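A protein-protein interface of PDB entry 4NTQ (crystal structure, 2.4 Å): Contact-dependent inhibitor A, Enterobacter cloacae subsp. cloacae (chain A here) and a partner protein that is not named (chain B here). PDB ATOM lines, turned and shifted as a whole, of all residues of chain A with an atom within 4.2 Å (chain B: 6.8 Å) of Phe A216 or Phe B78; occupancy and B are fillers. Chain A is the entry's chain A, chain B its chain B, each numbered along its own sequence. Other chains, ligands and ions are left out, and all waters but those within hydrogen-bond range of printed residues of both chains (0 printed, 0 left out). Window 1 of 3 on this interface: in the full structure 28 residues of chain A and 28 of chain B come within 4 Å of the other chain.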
ATOM      1  N   VAL A 192      -9.244  31.752   8.615  1.00  0.00           N
ATOM      2  CA  VAL A 192     -10.114  32.824   8.217  1.00  0.00           C
ATOM      3  C   VAL A 192      -9.318  34.107   8.512  1.00  0.00           C
ATOM      4  O   VAL A 192      -8.610  34.170   9.515  1.00  0.00           O
ATOM      5  CB  VAL A 192     -11.417  32.723   9.048  1.00  0.00           C
ATOM      6  CG1 VAL A 192     -11.891  34.052   9.487  1.00  0.00           C
ATOM      7  CG2 VAL A 192     -12.495  31.967   8.290  1.00  0.00           C
ATOM      8  N   ASN A 198     -15.102  42.166   8.442  1.00  0.00           N
ATOM      9  CA  ASN A 198     -15.429  40.951   7.702  1.00  0.00           C
ATOM     10  C   ASN A 198     -14.306  39.914   7.664  1.00  0.00           C
ATOM     11  O   ASN A 198     -13.165  40.195   8.058  1.00  0.00           O
ATOM     12  CB  ASN A 198     -15.813  41.310   6.271  1.00  0.00           C
ATOM     13  CG  ASN A 198     -17.111  42.057   6.201  1.00  0.00           C
ATOM     14  OD1 ASN A 198     -18.104  41.648   6.806  1.00  0.00           O
ATOM     15  ND2 ASN A 198     -17.118  43.166   5.468  1.00  0.00           N
ATOM     16  N   TYR A 199     -14.635  38.724   7.160  1.00  0.00           N
ATOM     17  CA  TYR A 199     -13.682  37.623   7.082  1.00  0.00           C
ATOM     18  C   TYR A 199     -13.552  37.087   5.660  1.00  0.00           C
ATOM     19  O   TYR A 199     -14.542  36.957   4.938  1.00  0.00           O
ATOM     20  CB  TYR A 199     -14.105  36.478   8.010  1.00  0.00           C
ATOM     21  CG  TYR A 199     -14.380  36.890   9.447  1.00  0.00           C
ATOM     22  CD1 TYR A 199     -13.405  36.755  10.435  1.00  0.00           C
ATOM     23  CD2 TYR A 199     -15.617  37.409   9.820  1.00  0.00           C
ATOM     24  CE1 TYR A 199     -13.654  37.114  11.752  1.00  0.00           C
ATOM     25  CE2 TYR A 199     -15.868  37.778  11.136  1.00  0.00           C
ATOM     26  CZ  TYR A 199     -14.880  37.639  12.094  1.00  0.00           C
ATOM     27  OH  TYR A 199     -15.132  38.016  13.393  1.00  0.00           O
ATOM     28  N   THR A 201     -11.603  33.850   3.265  1.00  0.00           N
ATOM     29  CA  THR A 201     -10.786  32.649   3.121  1.00  0.00           C
ATOM     30  C   THR A 201     -10.595  32.472   1.645  1.00  0.00           C
ATOM     31  O   THR A 201     -11.480  32.831   0.869  1.00  0.00           O
ATOM     32  CB  THR A 201     -11.480  31.352   3.586  1.00  0.00           C
ATOM     33  OG1 THR A 201     -12.676  31.141   2.825  1.00  0.00           O
ATOM     34  CG2 THR A 201     -11.824  31.407   5.024  1.00  0.00           C
ATOM     35  N   MET A 215     -16.171  35.512   1.183  1.00  0.00           N
ATOM     36  CA  MET A 215     -16.228  36.465   2.286  1.00  0.00           C
ATOM     37  C   MET A 215     -17.400  36.177   3.200  1.00  0.00           C
ATOM     38  O   MET A 215     -18.464  35.787   2.737  1.00  0.00           O
ATOM     39  CB  MET A 215     -16.313  37.891   1.758  1.00  0.00           C
ATOM     40  CG  MET A 215     -16.402  38.965   2.833  1.00  0.00           C
ATOM     41  SD  MET A 215     -16.431  40.756   2.053  1.00  0.00           S
ATOM     42  CE  MET A 215     -14.879  40.558   0.876  1.00  0.00           C
ATOM     43  N   PHE A 216     -17.201  36.362   4.501  1.00  0.00           N
ATOM     44  CA  PHE A 216     -18.278  36.196   5.465  1.00  0.00           C
ATOM     45  C   PHE A 216     -18.437  37.466   6.298  1.00  0.00           C
ATOM     46  O   PHE A 216     -17.452  38.120   6.640  1.00  0.00           O
ATOM     47  CB  PHE A 216     -18.007  34.999   6.374  1.00  0.00           C
ATOM     48  CG  PHE A 216     -17.841  33.702   5.635  1.00  0.00           C
ATOM     49  CD1 PHE A 216     -18.892  32.810   5.529  1.00  0.00           C
ATOM     50  CD2 PHE A 216     -16.635  33.377   5.042  1.00  0.00           C
ATOM     51  CE1 PHE A 216     -18.742  31.612   4.848  1.00  0.00           C
ATOM     52  CE2 PHE A 216     -16.473  32.176   4.367  1.00  0.00           C
ATOM     53  CZ  PHE A 216     -17.529  31.294   4.272  1.00  0.00           C
ATOM     54  N   ASN A 217     -19.670  37.827   6.627  1.00  0.00           N
ATOM     55  CA  ASN A 217     -19.860  39.061   7.389  1.00  0.00           C
ATOM     56  C   ASN A 217     -19.547  38.917   8.878  1.00  0.00           C
ATOM     57  O   ASN A 217     -19.117  37.848   9.323  1.00  0.00           O
ATOM     58  CB  ASN A 217     -21.239  39.685   7.144  1.00  0.00           C
ATOM     59  CG  ASN A 217     -22.369  38.904   7.772  1.00  0.00           C
ATOM     60  OD1 ASN A 217     -22.157  37.923   8.484  1.00  0.00           O
ATOM     61  ND2 ASN A 217     -23.590  39.350   7.516  1.00  0.00           N
ATOM     62  N   GLY A 220     -20.539  35.895  10.366  1.00  0.00           N
ATOM     63  CA  GLY A 220     -20.186  34.651   9.706  1.00  0.00           C
ATOM     64  C   GLY A 220     -21.147  34.224   8.611  1.00  0.00           C
ATOM     65  O   GLY A 220     -21.098  33.087   8.138  1.00  0.00           O
ATOM     66  N   LYS A 221     -22.043  35.121   8.214  1.00  0.00           N
ATOM     67  CA  LYS A 221     -22.899  34.852   7.064  1.00  0.00           C
ATOM     68  C   LYS A 221     -22.077  35.082   5.799  1.00  0.00           C
ATOM     69  O   LYS A 221     -21.360  36.086   5.697  1.00  0.00           O
ATOM     70  CB  LYS A 221     -24.102  35.786   7.060  1.00  0.00           C
ATOM     71  CG  LYS A 221     -24.925  35.786   8.333  1.00  0.00           C
ATOM     72  CD  LYS A 221     -26.027  34.737   8.302  1.00  0.00           C
ATOM     73  CE  LYS A 221     -26.953  34.901   9.496  1.00  0.00           C
ATOM     74  NZ  LYS A 221     -27.534  36.264   9.539  1.00  0.00           N
ATOM     75  N   ARG A 222     -22.173  34.163   4.840  1.00  0.00           N
ATOM     76  CA  ARG A 222     -21.493  34.333   3.556  1.00  0.00           C
ATOM     77  C   ARG A 222     -22.130  35.462   2.770  1.00  0.00           C
ATOM     78  O   ARG A 222     -23.352  35.484   2.574  1.00  0.00           O
ATOM     79  CB  ARG A 222     -21.572  33.056   2.740  1.00  0.00           C
ATOM     80  CG  ARG A 222     -20.810  33.078   1.420  1.00  0.00           C
ATOM     81  CD  ARG A 222     -20.646  31.645   0.902  1.00  0.00           C
ATOM     82  NE  ARG A 222     -20.304  31.571  -0.516  1.00  0.00           N
ATOM     83  CZ  ARG A 222     -20.016  30.435  -1.155  1.00  0.00           C
ATOM     84  NH1 ARG A 222     -20.022  29.279  -0.492  1.00  0.00           N
ATOM     85  NH2 ARG A 222     -19.724  30.454  -2.455  1.00  0.00           N
ATOM     86  N   LEU B  32     -15.169  20.946  -1.237  1.00  0.00           N
ATOM     87  CA  LEU B  32     -14.872  21.117   0.186  1.00  0.00           C
ATOM     88  C   LEU B  32     -13.727  20.195   0.629  1.00  0.00           C
ATOM     89  O   LEU B  32     -13.509  19.119   0.045  1.00  0.00           O
ATOM     90  CB  LEU B  32     -16.108  20.821   1.029  1.00  0.00           C
ATOM     91  CG  LEU B  32     -17.368  21.643   0.744  1.00  0.00           C
ATOM     92  CD1 LEU B  32     -18.519  21.028   1.496  1.00  0.00           C
ATOM     93  CD2 LEU B  32     -17.157  23.118   1.142  1.00  0.00           C
ATOM     94  N   TYR B  44     -18.988  12.714  10.592  1.00  0.00           N
ATOM     95  CA  TYR B  44     -19.606  13.835   9.904  1.00  0.00           C
ATOM     96  C   TYR B  44     -20.998  13.411   9.508  1.00  0.00           C
ATOM     97  O   TYR B  44     -21.972  14.141   9.722  1.00  0.00           O
ATOM     98  CB  TYR B  44     -18.827  14.222   8.648  1.00  0.00           C
ATOM     99  CG  TYR B  44     -17.680  15.189   8.875  1.00  0.00           C
ATOM    100  CD1 TYR B  44     -17.909  16.567   8.970  1.00  0.00           C
ATOM    101  CD2 TYR B  44     -16.363  14.731   8.968  1.00  0.00           C
ATOM    102  CE1 TYR B  44     -16.849  17.466   9.177  1.00  0.00           C
ATOM    103  CE2 TYR B  44     -15.304  15.614   9.168  1.00  0.00           C
ATOM    104  CZ  TYR B  44     -15.546  16.980   9.276  1.00  0.00           C
ATOM    105  OH  TYR B  44     -14.489  17.853   9.480  1.00  0.00           O
ATOM    106  N   LEU B  64     -25.440  21.578   8.810  1.00  0.00           N
ATOM    107  CA  LEU B  64     -24.522  20.504   8.425  1.00  0.00           C
ATOM    108  C   LEU B  64     -23.085  20.995   8.513  1.00  0.00           C
ATOM    109  O   LEU B  64     -22.640  21.742   7.642  1.00  0.00           O
ATOM    110  CB  LEU B  64     -24.767  20.076   6.973  1.00  0.00           C
ATOM    111  CG  LEU B  64     -26.189  19.703   6.568  1.00  0.00           C
ATOM    112  CD1 LEU B  64     -26.268  19.363   5.082  1.00  0.00           C
ATOM    113  CD2 LEU B  64     -26.683  18.546   7.390  1.00  0.00           C
ATOM    114  N   ALA B  65     -22.354  20.564   9.537  1.00  0.00           N
ATOM    115  CA  ALA B  65     -20.969  20.991   9.715  1.00  0.00           C
ATOM    116  C   ALA B  65     -20.060  20.357   8.660  1.00  0.00           C
ATOM    117  O   ALA B  65     -20.176  19.169   8.361  1.00  0.00           O
ATOM    118  CB  ALA B  65     -20.473  20.631  11.106  1.00  0.00           C
ATOM    119  N   VAL B  66     -19.164  21.149   8.086  1.00  0.00           N
ATOM    120  CA  VAL B  66     -18.194  20.588   7.152  1.00  0.00           C
ATOM    121  C   VAL B  66     -16.768  20.862   7.626  1.00  0.00           C
ATOM    122  O   VAL B  66     -15.803  20.801   6.856  1.00  0.00           O
ATOM    123  CB  VAL B  66     -18.436  21.066   5.730  1.00  0.00           C
ATOM    124  CG1 VAL B  66     -19.810  20.566   5.259  1.00  0.00           C
ATOM    125  CG2 VAL B  66     -18.328  22.566   5.666  1.00  0.00           C
ATOM    126  N   SER B  67     -16.657  21.171   8.914  1.00  0.00           N
ATOM    127  CA  SER B  67     -15.382  21.122   9.596  1.00  0.00           C
ATOM    128  C   SER B  67     -15.689  20.989  11.076  1.00  0.00           C
ATOM    129  O   SER B  67     -16.713  21.478  11.547  1.00  0.00           O
ATOM    130  CB  SER B  67     -14.540  22.379   9.323  1.00  0.00           C
ATOM    131  OG  SER B  67     -15.097  23.509   9.974  1.00  0.00           O
ATOM    132  N   MET B  68     -14.793  20.329  11.802  1.00  0.00           N
ATOM    133  CA  MET B  68     -14.973  20.089  13.210  1.00  0.00           C
ATOM    134  C   MET B  68     -13.627  19.778  13.823  1.00  0.00           C
ATOM    135  O   MET B  68     -12.797  19.092  13.220  1.00  0.00           O
ATOM    136  CB  MET B  68     -15.921  18.915  13.436  1.00  0.00           C
ATOM    137  CG  MET B  68     -16.202  18.634  14.904  1.00  0.00           C
ATOM    138  SD  MET B  68     -17.110  20.157  15.751  1.00  0.00           S
ATOM    139  CE  MET B  68     -18.373  20.552  14.291  1.00  0.00           C
ATOM    140  N   PHE B  76     -13.786  28.238  15.221  1.00  0.00           N
ATOM    141  CA  PHE B  76     -14.925  28.354  14.308  1.00  0.00           C
ATOM    142  C   PHE B  76     -15.075  27.108  13.435  1.00  0.00           C
ATOM    143  O   PHE B  76     -14.120  26.373  13.232  1.00  0.00           O
ATOM    144  CB  PHE B  76     -14.754  29.568  13.401  1.00  0.00           C
ATOM    145  CG  PHE B  76     -13.538  29.494  12.509  1.00  0.00           C
ATOM    146  CD1 PHE B  76     -13.617  28.917  11.250  1.00  0.00           C
ATOM    147  CD2 PHE B  76     -12.331  30.017  12.921  1.00  0.00           C
ATOM    148  CE1 PHE B  76     -12.508  28.858  10.428  1.00  0.00           C
ATOM    149  CE2 PHE B  76     -11.224  29.971  12.109  1.00  0.00           C
ATOM    150  CZ  PHE B  76     -11.309  29.384  10.860  1.00  0.00           C
ATOM    151  N   ILE B  77     -16.271  26.880  12.916  1.00  0.00           N
ATOM    152  CA  ILE B  77     -16.493  25.779  12.001  1.00  0.00           C
ATOM    153  C   ILE B  77     -17.320  26.263  10.824  1.00  0.00           C
ATOM    154  O   ILE B  77     -18.131  27.184  10.966  1.00  0.00           O
ATOM    155  CB  ILE B  77     -17.242  24.619  12.675  1.00  0.00           C
ATOM    156  CG1 ILE B  77     -18.648  25.066  13.092  1.00  0.00           C
ATOM    157  CG2 ILE B  77     -16.445  24.083  13.863  1.00  0.00           C
ATOM    158  CD1 ILE B  77     -19.507  23.983  13.711  1.00  0.00           C
ATOM    159  N   PHE B  78     -17.090  25.664   9.658  1.00  0.00           N
ATOM    160  CA  PHE B  78     -17.903  25.954   8.483  1.00  0.00           C
ATOM    161  C   PHE B  78     -19.115  25.056   8.495  1.00  0.00           C
ATOM    162  O   PHE B  78     -19.021  23.877   8.842  1.00  0.00           O
ATOM    163  CB  PHE B  78     -17.119  25.757   7.183  1.00  0.00           C
ATOM    164  CG  PHE B  78     -16.017  26.752   6.989  1.00  0.00           C
ATOM    165  CD1 PHE B  78     -16.261  27.958   6.359  1.00  0.00           C
ATOM    166  CD2 PHE B  78     -14.742  26.485   7.449  1.00  0.00           C
ATOM    167  CE1 PHE B  78     -15.249  28.874   6.181  1.00  0.00           C
ATOM    168  CE2 PHE B  78     -13.726  27.403   7.279  1.00  0.00           C
ATOM    169  CZ  PHE B  78     -13.980  28.601   6.644  1.00  0.00           C
ATOM    170  N   THR B  79     -20.262  25.623   8.141  1.00  0.00           N
ATOM    171  CA  THR B  79     -21.483  24.850   8.056  1.00  0.00           C
ATOM    172  C   THR B  79     -22.245  25.210   6.804  1.00  0.00           C
ATOM    173  O   THR B  79     -22.073  26.295   6.241  1.00  0.00           O
ATOM    174  CB  THR B  79     -22.415  25.153   9.229  1.00  0.00           C
ATOM    175  OG1 THR B  79     -22.875  26.503   9.114  1.00  0.00           O
ATOM    176  CG2 THR B  79     -21.697  24.959  10.572  1.00  0.00           C
ATOM    177  N   TRP B  80     -23.088  24.283   6.367  1.00  0.00           N
ATOM    178  CA  TRP B  80     -24.102  24.587   5.376  1.00  0.00           C
ATOM    179  C   TRP B  80     -25.428  24.393   6.085  1.00  0.00           C
ATOM    180  O   TRP B  80     -25.648  23.360   6.723  1.00  0.00           O
ATOM    181  CB  TRP B  80     -23.935  23.712   4.131  1.00  0.00           C
ATOM    182  CG  TRP B  80     -22.688  24.141   3.357  1.00  0.00           C
ATOM    183  CD1 TRP B  80     -21.392  23.874   3.688  1.00  0.00           C
ATOM    184  CD2 TRP B  80     -22.636  24.972   2.182  1.00  0.00           C
ATOM    185  NE1 TRP B  80     -20.540  24.465   2.783  1.00  0.00           N
ATOM    186  CE2 TRP B  80     -21.275  25.138   1.848  1.00  0.00           C
ATOM    187  CE3 TRP B  80     -23.611  25.583   1.375  1.00  0.00           C
ATOM    188  CZ2 TRP B  80     -20.861  25.886   0.745  1.00  0.00           C
ATOM    189  CZ3 TRP B  80     -23.200  26.321   0.280  1.00  0.00           C
ATOM    190  CH2 TRP B  80     -21.834  26.474  -0.022  1.00  0.00           C
ATOM    191  N   ASN B  93     -24.413  29.297   3.673  1.00  0.00           N
ATOM    192  CA  ASN B  93     -23.102  28.799   4.036  1.00  0.00           C
ATOM    193  C   ASN B  93     -22.606  29.745   5.096  1.00  0.00           C
ATOM    194  O   ASN B  93     -22.290  30.900   4.807  1.00  0.00           O
ATOM    195  CB  ASN B  93     -22.195  28.802   2.788  1.00  0.00           C
ATOM    196  CG  ASN B  93     -20.740  28.425   3.090  1.00  0.00           C
ATOM    197  OD1 ASN B  93     -19.820  28.939   2.440  1.00  0.00           O
ATOM    198  ND2 ASN B  93     -20.526  27.520   4.061  1.00  0.00           N
ATOM    199  N   ASN B  94     -22.596  29.278   6.340  1.00  0.00           N
ATOM    200  CA  ASN B  94     -22.344  30.166   7.473  1.00  0.00           C
ATOM    201  C   ASN B  94     -21.193  29.662   8.279  1.00  0.00           C
ATOM    202  O   ASN B  94     -21.052  28.453   8.475  1.00  0.00           O
ATOM    203  CB  ASN B  94     -23.598  30.304   8.363  1.00  0.00           C
ATOM    204  CG  ASN B  94     -24.778  30.896   7.611  1.00  0.00           C
ATOM    205  OD1 ASN B  94     -24.604  31.552   6.577  1.00  0.00           O
ATOM    206  ND2 ASN B  94     -25.984  30.672   8.120  1.00  0.00           N
ATOM    207  N   VAL B  95     -20.350  30.584   8.723  1.00  0.00           N
ATOM    208  CA  VAL B  95     -19.276  30.251   9.643  1.00  0.00           C
ATOM    209  C   VAL B  95     -19.767  30.495  11.055  1.00  0.00           C
ATOM    210  O   VAL B  95     -20.227  31.598  11.368  1.00  0.00           O
ATOM    211  CB  VAL B  95     -18.051  31.130   9.418  1.00  0.00           C
ATOM    212  CG1 VAL B  95     -17.022  30.870  10.486  1.00  0.00           C
ATOM    213  CG2 VAL B  95     -17.473  30.879   8.055  1.00  0.00           C
ATOM    214  N   ILE B  96     -19.676  29.477  11.903  1.00  0.00           N
ATOM    215  CA  ILE B  96     -20.032  29.642  13.300  1.00  0.00           C
ATOM    216  C   ILE B  96     -18.811  29.964  14.161  1.00  0.00           C
ATOM    217  O   ILE B  96     -17.920  29.135  14.312  1.00  0.00           O
ATOM    218  CB  ILE B  96     -20.669  28.390  13.860  1.00  0.00           C
ATOM    219  CG1 ILE B  96     -21.839  27.943  12.993  1.00  0.00           C
ATOM    220  CG2 ILE B  96     -21.147  28.656  15.254  1.00  0.00           C
ATOM    221  CD1 ILE B  96     -22.725  26.947  13.696  1.00  0.00           C
ATOM    222  N   PHE B  97     -18.787  31.160  14.743  1.00  0.00           N
ATOM    223  CA  PHE B  97     -17.666  31.583  15.579  1.00  0.00           C
ATOM    224  C   PHE B  97     -17.825  31.136  17.021  1.00  0.00           C
ATOM    225  O   PHE B  97     -18.870  31.337  17.623  1.00  0.00           O
ATOM    226  CB  PHE B  97     -17.493  33.097  15.516  1.00  0.00           C
ATOM    227  CG  PHE B  97     -16.856  33.565  14.251  1.00  0.00           C
ATOM    228  CD1 PHE B  97     -15.517  33.318  14.013  1.00  0.00           C
ATOM    229  CD2 PHE B  97     -17.592  34.236  13.296  1.00  0.00           C
ATOM    230  CE1 PHE B  97     -14.920  33.738  12.839  1.00  0.00           C
ATOM    231  CE2 PHE B  97     -17.002  34.655  12.121  1.00  0.00           C
ATOM    232  CZ  PHE B  97     -15.670  34.408  11.890  1.00  0.00           C
ATOM    233  N   ILE B 109     -25.512  21.694  17.624  1.00  0.00           N
ATOM    234  CA  ILE B 109     -25.257  22.621  16.515  1.00  0.00           C
ATOM    235  C   ILE B 109     -26.484  23.427  16.040  1.00  0.00           C
ATOM    236  O   ILE B 109     -26.359  24.580  15.632  1.00  0.00           O
ATOM    237  CB  ILE B 109     -24.593  21.902  15.307  1.00  0.00           C
ATOM    238  CG1 ILE B 109     -24.177  22.901  14.228  1.00  0.00           C
ATOM    239  CG2 ILE B 109     -25.527  20.888  14.701  1.00  0.00           C
ATOM    240  CD1 ILE B 109     -23.444  22.267  13.031  1.00  0.00           C
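The backbone NH (N) of Val B95 is in hydrogen-bond range of the backbone carbonyl oxygen (O) of Gly A220, at 2.7 Å.
The side-chain amide oxygen (OD1) of Asn B93 lies within hydrogen-bond range of the guanidinium group (NH1) of Arg A222 (3.0 Å).
ND2 of Asn B93 sits close to NE1 of Trp B80 (3.3 Å).
The backbone NH (N) of Phe B78 sits at hydrogen-bond distance from the side-chain hydroxyl (OG) of Ser B67.
The side-chain amide oxygen of Asn A217 lies within hydrogen-bond range of the backbone NH of Lys A221 (2.8 Å).
The side-chain amide nitrogen of Asn B93 is in hydrogen-bond range of the backbone carbonyl oxygen of Thr B79, 2.9 Å away.
N of Val B66 is in hydrogen-bond range of O of Phe B78, at 2.8 Å.
The side-chain amide oxygen of Asn A217 is in hydrogen-bond range of the backbone NH of Gly A220, at 3.2 Å.
Phe B76 touches Val A192.
Phe B78 touches Thr A201 (CZ to CG2, 3.9 Å).
CZ of Phe A216 touches CE1 of Phe B78 (3.8 Å).
Phe A216 touches Asn B93 (CE1 to O, 3.6 Å).
CD1 of Phe A216 touches CG2 of Val B95, at 3.5 Å.
O of Gly A220 touches CA of Asn B94, 3.2 Å away.
CA of Gly A220 touches CE2 of Phe B97 (3.996 Å).
Lys A221 touches Asn B94.
NH1 of Arg A222 touches CH2 of Trp B80 (3.4 Å).
Asn B94 touches Arg A222 (OD1 to N, 3.97 Å).
Of the printed residues of chain B, Tyr A199 touches Phe B97 (3.3 Å).
Of the printed residues of chain B, Thr A201 touches Phe B78 (3.9 Å).
Phe B78 touches just these residues of chain A: Thr A201 (3.9 Å) and Phe A216 (3.8 Å).
Hydrophobic or aromatic side chains of chain B within 4 Å of the printed part of chain A: Phe B76, Phe B78, Trp B80, Val B95 and Phe B97.
Among the printed residues, no Asp or Glu carboxylate lies within 4 Å of a Lys or Arg side-chain nitrogen of the other chain.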
